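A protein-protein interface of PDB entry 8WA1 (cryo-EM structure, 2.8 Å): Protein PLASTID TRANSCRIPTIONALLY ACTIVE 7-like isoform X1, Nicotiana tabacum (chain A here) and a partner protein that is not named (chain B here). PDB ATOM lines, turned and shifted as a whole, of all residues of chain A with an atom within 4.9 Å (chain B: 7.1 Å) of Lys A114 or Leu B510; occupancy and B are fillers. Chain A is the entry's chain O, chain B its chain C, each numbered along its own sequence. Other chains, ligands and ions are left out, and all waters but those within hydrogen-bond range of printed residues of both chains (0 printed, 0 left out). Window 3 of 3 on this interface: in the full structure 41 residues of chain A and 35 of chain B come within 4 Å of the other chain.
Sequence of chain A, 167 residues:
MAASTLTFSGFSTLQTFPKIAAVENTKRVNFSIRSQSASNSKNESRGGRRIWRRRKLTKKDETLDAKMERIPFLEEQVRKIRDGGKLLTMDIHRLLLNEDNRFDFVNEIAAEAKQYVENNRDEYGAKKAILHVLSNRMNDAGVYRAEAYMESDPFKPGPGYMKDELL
Of the 11 printed residues of chain B, 5 touch a printed residue of chain A.
Hydrophobic or aromatic side chains of chain B that line the printed part of chain A: Leu B510 and Val B514.
Of the 11 printed residues of chain A, 6 touch a printed residue of chain B.
Hydrophobic or aromatic side chains of chain A within 4 Å of the printed part of chain B: Ile A109, Ala A110, Val A117 and Ile A130.
Among the printed residues, 9 pairs touch across the chains.
Among the printed residues, no Asp or Glu carboxylate lies within 4 Å of a Lys or Arg side-chain nitrogen of the other chain.
Among the printed residues, merely in contact across the chains: Ile A130 with Arg B517 (3.3 Å), Ile A130 with Gln B513 (3.6 Å), Ile A130 with Val B514 (3.6 Å), Ala A110 with Glu B511 (3.6 Å), Val A117 with Leu B510 (3.7 Å), Ile A109 with Val B514 (3.8 Å), Lys A114 with Leu B510 (3.9 Å), Ile A130 with Leu B510 (3.97 Å) and Ala A113 with Leu B510 (3.97 Å).
Of the printed residues of chain B, Ala A110 touches Glu B511.
Glu A112 touches none of the printed residues of chain B.
Of chain B, only Leu B510 comes within 4 Å of Lys A114.
Of the printed residues of chain B, Val A117 touches Leu B510 (3.7 Å).
Ser B509 touches none of the printed residues of chain A.
Printed residues of chain A within 4 Å of Leu B510: Ala A113 (3.97 Å), Lys A114 (3.9 Å), Val A117 (3.7 Å) and Ile A130 (3.97 Å).
The nearest residue of chain B that does not touch Lys A114 is Glu B511 (4.5 Å).
The nearest printed residue of chain A that does not touch Arg B517 is Ile A109 (6.8 Å).
The backbone carbonyl oxygen of Leu B508 lies close to the side-chain amide oxygen of Gln B513, at 3.3 Å.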
ATOM      1  N   ILE A 109      14.683 -14.845 -12.773  1.00  0.00           N
ATOM      2  CA  ILE A 109      13.906 -15.222 -13.951  1.00  0.00           C
ATOM      3  C   ILE A 109      13.244 -16.576 -13.737  1.00  0.00           C
ATOM      4  O   ILE A 109      12.085 -16.784 -14.120  1.00  0.00           O
ATOM      5  CB  ILE A 109      14.798 -15.221 -15.207  1.00  0.00           C
ATOM      6  CG1 ILE A 109      15.234 -13.798 -15.553  1.00  0.00           C
ATOM      7  CG2 ILE A 109      14.068 -15.846 -16.386  1.00  0.00           C
ATOM      8  CD1 ILE A 109      16.011 -13.712 -16.842  1.00  0.00           C
ATOM      9  N   ALA A 110      13.963 -17.515 -13.118  1.00  0.00           N
ATOM     10  CA  ALA A 110      13.389 -18.830 -12.851  1.00  0.00           C
ATOM     11  C   ALA A 110      12.202 -18.731 -11.901  1.00  0.00           C
ATOM     12  O   ALA A 110      11.171 -19.377 -12.118  1.00  0.00           O
ATOM     13  CB  ALA A 110      14.459 -19.761 -12.282  1.00  0.00           C
ATOM     14  N   ALA A 111      12.326 -17.923 -10.847  1.00  0.00           N
ATOM     15  CA  ALA A 111      11.222 -17.760  -9.906  1.00  0.00           C
ATOM     16  C   ALA A 111      10.019 -17.099 -10.572  1.00  0.00           C
ATOM     17  O   ALA A 111       8.872 -17.503 -10.336  1.00  0.00           O
ATOM     18  CB  ALA A 111      11.679 -16.948  -8.695  1.00  0.00           C
ATOM     19  N   GLU A 112      10.259 -16.090 -11.411  1.00  0.00           N
ATOM     20  CA  GLU A 112       9.151 -15.422 -12.089  1.00  0.00           C
ATOM     21  C   GLU A 112       8.461 -16.359 -13.074  1.00  0.00           C
ATOM     22  O   GLU A 112       7.228 -16.359 -13.179  1.00  0.00           O
ATOM     23  CB  GLU A 112       9.652 -14.164 -12.797  1.00  0.00           C
ATOM     24  CG  GLU A 112       8.544 -13.273 -13.329  1.00  0.00           C
ATOM     25  CD  GLU A 112       9.052 -11.917 -13.780  1.00  0.00           C
ATOM     26  OE1 GLU A 112      10.273 -11.675 -13.678  1.00  0.00           O
ATOM     27  OE2 GLU A 112       8.230 -11.092 -14.232  1.00  0.00           O
ATOM     28  N   ALA A 113       9.236 -17.174 -13.795  1.00  0.00           N
ATOM     29  CA  ALA A 113       8.639 -18.150 -14.698  1.00  0.00           C
ATOM     30  C   ALA A 113       7.870 -19.219 -13.937  1.00  0.00           C
ATOM     31  O   ALA A 113       6.820 -19.677 -14.404  1.00  0.00           O
ATOM     32  CB  ALA A 113       9.720 -18.791 -15.568  1.00  0.00           C
ATOM     33  N   LYS A 114       8.364 -19.622 -12.764  1.00  0.00           N
ATOM     34  CA  LYS A 114       7.626 -20.573 -11.940  1.00  0.00           C
ATOM     35  C   LYS A 114       6.299 -19.984 -11.483  1.00  0.00           C
ATOM     36  O   LYS A 114       5.270 -20.669 -11.495  1.00  0.00           O
ATOM     37  CB  LYS A 114       8.473 -20.994 -10.738  1.00  0.00           C
ATOM     38  CG  LYS A 114       7.766 -21.934  -9.774  1.00  0.00           C
ATOM     39  CD  LYS A 114       8.660 -22.286  -8.596  1.00  0.00           C
ATOM     40  CE  LYS A 114       7.929 -23.152  -7.582  1.00  0.00           C
ATOM     41  NZ  LYS A 114       7.479 -24.444  -8.170  1.00  0.00           N
ATOM     42  N   GLN A 115       6.304 -18.712 -11.076  1.00  0.00           N
ATOM     43  CA  GLN A 115       5.052 -18.055 -10.708  1.00  0.00           C
ATOM     44  C   GLN A 115       4.097 -17.985 -11.892  1.00  0.00           C
ATOM     45  O   GLN A 115       2.894 -18.241 -11.746  1.00  0.00           O
ATOM     46  CB  GLN A 115       5.328 -16.656 -10.157  1.00  0.00           C
ATOM     47  CG  GLN A 115       5.827 -16.637  -8.722  1.00  0.00           C
ATOM     48  CD  GLN A 115       5.941 -15.231  -8.164  1.00  0.00           C
ATOM     49  OE1 GLN A 115       6.203 -15.041  -6.977  1.00  0.00           O
ATOM     50  NE2 GLN A 115       5.744 -14.235  -9.022  1.00  0.00           N
ATOM     51  N   TYR A 116       4.611 -17.638 -13.075  1.00  0.00           N
ATOM     52  CA  TYR A 116       3.765 -17.582 -14.266  1.00  0.00           C
ATOM     53  C   TYR A 116       3.151 -18.942 -14.577  1.00  0.00           C
ATOM     54  O   TYR A 116       1.971 -19.032 -14.935  1.00  0.00           O
ATOM     55  CB  TYR A 116       4.566 -17.075 -15.466  1.00  0.00           C
ATOM     56  CG  TYR A 116       4.701 -15.571 -15.539  1.00  0.00           C
ATOM     57  CD1 TYR A 116       4.428 -14.773 -14.435  1.00  0.00           C
ATOM     58  CD2 TYR A 116       5.106 -14.951 -16.712  1.00  0.00           C
ATOM     59  CE1 TYR A 116       4.553 -13.398 -14.502  1.00  0.00           C
ATOM     60  CE2 TYR A 116       5.232 -13.577 -16.787  1.00  0.00           C
ATOM     61  CZ  TYR A 116       4.956 -12.806 -15.680  1.00  0.00           C
ATOM     62  OH  TYR A 116       5.081 -11.438 -15.752  1.00  0.00           O
ATOM     63  N   VAL A 117       3.941 -20.012 -14.455  1.00  0.00           N
ATOM     64  CA  VAL A 117       3.425 -21.350 -14.727  1.00  0.00           C
ATOM     65  C   VAL A 117       2.375 -21.740 -13.695  1.00  0.00           C
ATOM     66  O   VAL A 117       1.325 -22.297 -14.037  1.00  0.00           O
ATOM     67  CB  VAL A 117       4.583 -22.366 -14.773  1.00  0.00           C
ATOM     68  CG1 VAL A 117       4.048 -23.789 -14.732  1.00  0.00           C
ATOM     69  CG2 VAL A 117       5.419 -22.151 -16.022  1.00  0.00           C
ATOM     70  N   GLU A 118       2.630 -21.444 -12.418  1.00  0.00           N
ATOM     71  CA  GLU A 118       1.679 -21.802 -11.371  1.00  0.00           C
ATOM     72  C   GLU A 118       0.381 -21.016 -11.507  1.00  0.00           C
ATOM     73  O   GLU A 118      -0.689 -21.499 -11.116  1.00  0.00           O
ATOM     74  CB  GLU A 118       2.303 -21.575  -9.994  1.00  0.00           C
ATOM     75  CG  GLU A 118       2.554 -22.852  -9.206  1.00  0.00           C
ATOM     76  CD  GLU A 118       3.597 -23.746  -9.850  1.00  0.00           C
ATOM     77  OE1 GLU A 118       4.463 -23.224 -10.583  1.00  0.00           O
ATOM     78  OE2 GLU A 118       3.551 -24.973  -9.621  1.00  0.00           O
ATOM     79  N   ILE A 130       9.370 -18.639 -19.797  1.00  0.00           N
ATOM     80  CA  ILE A 130      10.604 -17.870 -19.669  1.00  0.00           C
ATOM     81  C   ILE A 130      10.681 -16.807 -20.757  1.00  0.00           C
ATOM     82  O   ILE A 130      11.038 -15.648 -20.496  1.00  0.00           O
ATOM     83  CB  ILE A 130      11.818 -18.814 -19.704  1.00  0.00           C
ATOM     84  CG1 ILE A 130      11.585 -19.989 -18.752  1.00  0.00           C
ATOM     85  CG2 ILE A 130      13.086 -18.064 -19.333  1.00  0.00           C
ATOM     86  CD1 ILE A 130      12.451 -21.190 -19.031  1.00  0.00           C
ATOM     87  N   PRO B 507      16.859 -30.228 -20.534  1.00  0.00           N
ATOM     88  CA  PRO B 507      16.520 -29.752 -19.185  1.00  0.00           C
ATOM     89  C   PRO B 507      15.024 -29.768 -18.912  1.00  0.00           C
ATOM     90  O   PRO B 507      14.246 -29.155 -19.649  1.00  0.00           O
ATOM     91  CB  PRO B 507      17.074 -28.320 -19.171  1.00  0.00           C
ATOM     92  CG  PRO B 507      18.057 -28.267 -20.301  1.00  0.00           C
ATOM     93  CD  PRO B 507      17.497 -29.177 -21.341  1.00  0.00           C
ATOM     94  N   LEU B 508      14.613 -30.479 -17.861  1.00  0.00           N
ATOM     95  CA  LEU B 508      13.191 -30.581 -17.541  1.00  0.00           C
ATOM     96  C   LEU B 508      12.713 -29.392 -16.715  1.00  0.00           C
ATOM     97  O   LEU B 508      11.680 -28.789 -17.027  1.00  0.00           O
ATOM     98  CB  LEU B 508      12.911 -31.889 -16.800  1.00  0.00           C
ATOM     99  CG  LEU B 508      12.633 -33.158 -17.610  1.00  0.00           C
ATOM    100  CD1 LEU B 508      11.398 -32.971 -18.476  1.00  0.00           C
ATOM    101  CD2 LEU B 508      13.829 -33.570 -18.457  1.00  0.00           C
ATOM    102  N   SER B 509      13.440 -29.049 -15.654  1.00  0.00           N
ATOM    103  CA  SER B 509      13.004 -28.008 -14.738  1.00  0.00           C
ATOM    104  C   SER B 509      13.136 -26.629 -15.380  1.00  0.00           C
ATOM    105  O   SER B 509      13.953 -26.406 -16.276  1.00  0.00           O
ATOM    106  CB  SER B 509      13.810 -28.060 -13.440  1.00  0.00           C
ATOM    107  OG  SER B 509      13.631 -29.299 -12.777  1.00  0.00           O
ATOM    108  N   LEU B 510      12.310 -25.695 -14.901  1.00  0.00           N
ATOM    109  CA  LEU B 510      12.344 -24.336 -15.431  1.00  0.00           C
ATOM    110  C   LEU B 510      13.655 -23.642 -15.085  1.00  0.00           C
ATOM    111  O   LEU B 510      14.201 -22.891 -15.903  1.00  0.00           O
ATOM    112  CB  LEU B 510      11.157 -23.534 -14.899  1.00  0.00           C
ATOM    113  CG  LEU B 510       9.770 -24.020 -15.322  1.00  0.00           C
ATOM    114  CD1 LEU B 510       8.686 -23.175 -14.675  1.00  0.00           C
ATOM    115  CD2 LEU B 510       9.639 -23.998 -16.835  1.00  0.00           C
ATOM    116  N   GLU B 511      14.168 -23.870 -13.874  1.00  0.00           N
ATOM    117  CA  GLU B 511      15.453 -23.289 -13.495  1.00  0.00           C
ATOM    118  C   GLU B 511      16.565 -23.787 -14.409  1.00  0.00           C
ATOM    119  O   GLU B 511      17.427 -23.008 -14.836  1.00  0.00           O
ATOM    120  CB  GLU B 511      15.777 -23.618 -12.036  1.00  0.00           C
ATOM    121  CG  GLU B 511      14.734 -23.156 -11.027  1.00  0.00           C
ATOM    122  CD  GLU B 511      13.575 -24.124 -10.894  1.00  0.00           C
ATOM    123  OE1 GLU B 511      13.627 -25.203 -11.521  1.00  0.00           O
ATOM    124  OE2 GLU B 511      12.611 -23.806 -10.167  1.00  0.00           O
ATOM    125  N   ALA B 512      16.558 -25.085 -14.723  1.00  0.00           N
ATOM    126  CA  ALA B 512      17.557 -25.631 -15.633  1.00  0.00           C
ATOM    127  C   ALA B 512      17.424 -25.029 -17.025  1.00  0.00           C
ATOM    128  O   ALA B 512      18.430 -24.760 -17.691  1.00  0.00           O
ATOM    129  CB  ALA B 512      17.436 -27.154 -15.692  1.00  0.00           C
ATOM    130  N   GLN B 513      16.189 -24.804 -17.481  1.00  0.00           N
ATOM    131  CA  GLN B 513      15.987 -24.188 -18.788  1.00  0.00           C
ATOM    132  C   GLN B 513      16.515 -22.760 -18.813  1.00  0.00           C
ATOM    133  O   GLN B 513      17.157 -22.345 -19.786  1.00  0.00           O
ATOM    134  CB  GLN B 513      14.505 -24.218 -19.163  1.00  0.00           C
ATOM    135  CG  GLN B 513      13.939 -25.613 -19.358  1.00  0.00           C
ATOM    136  CD  GLN B 513      12.461 -25.598 -19.686  1.00  0.00           C
ATOM    137  OE1 GLN B 513      11.748 -26.570 -19.438  1.00  0.00           O
ATOM    138  NE2 GLN B 513      11.992 -24.492 -20.252  1.00  0.00           N
ATOM    139  N   VAL B 514      16.255 -21.991 -17.754  1.00  0.00           N
ATOM    140  CA  VAL B 514      16.769 -20.625 -17.682  1.00  0.00           C
ATOM    141  C   VAL B 514      18.291 -20.630 -17.671  1.00  0.00           C
ATOM    142  O   VAL B 514      18.936 -19.830 -18.363  1.00  0.00           O
ATOM    143  CB  VAL B 514      16.197 -19.897 -16.450  1.00  0.00           C
ATOM    144  CG1 VAL B 514      16.781 -18.499 -16.344  1.00  0.00           C
ATOM    145  CG2 VAL B 514      14.685 -19.830 -16.525  1.00  0.00           C
ATOM    146  N   GLU B 515      18.889 -21.528 -16.881  1.00  0.00           N
ATOM    147  CA  GLU B 515      20.345 -21.627 -16.841  1.00  0.00           C
ATOM    148  C   GLU B 515      20.916 -21.956 -18.214  1.00  0.00           C
ATOM    149  O   GLU B 515      21.880 -21.326 -18.661  1.00  0.00           O
ATOM    150  CB  GLU B 515      20.772 -22.681 -15.821  1.00  0.00           C
ATOM    151  CG  GLU B 515      20.531 -22.292 -14.375  1.00  0.00           C
ATOM    152  CD  GLU B 515      20.964 -23.371 -13.405  1.00  0.00           C
ATOM    153  OE1 GLU B 515      21.364 -24.462 -13.863  1.00  0.00           O
ATOM    154  OE2 GLU B 515      20.906 -23.129 -12.183  1.00  0.00           O
ATOM    155  N   ALA B 516      20.324 -22.934 -18.901  1.00  0.00           N
ATOM    156  CA  ALA B 516      20.821 -23.327 -20.216  1.00  0.00           C
ATOM    157  C   ALA B 516      20.678 -22.192 -21.221  1.00  0.00           C
ATOM    158  O   ALA B 516      21.565 -21.966 -22.050  1.00  0.00           O
ATOM    159  CB  ALA B 516      20.080 -24.572 -20.701  1.00  0.00           C
ATOM    160  N   ARG B 517      19.562 -21.462 -21.161  1.00  0.00           N
ATOM    161  CA  ARG B 517      19.317 -20.417 -22.148  1.00  0.00           C
ATOM    162  C   ARG B 517      20.174 -19.182 -21.900  1.00  0.00           C
ATOM    163  O   ARG B 517      20.546 -18.491 -22.856  1.00  0.00           O
ATOM    164  CB  ARG B 517      17.835 -20.042 -22.154  1.00  0.00           C
ATOM    165  CG  ARG B 517      17.434 -19.100 -23.277  1.00  0.00           C
ATOM    166  CD  ARG B 517      15.931 -18.852 -23.293  1.00  0.00           C
ATOM    167  NE  ARG B 517      15.170 -20.069 -23.566  1.00  0.00           N
ATOM    168  CZ  ARG B 517      14.578 -20.807 -22.631  1.00  0.00           C
ATOM    169  NH1 ARG B 517      14.656 -20.452 -21.357  1.00  0.00           N
ATOM    170  NH2 ARG B 517      13.908 -21.899 -22.972  1.00  0.00           N
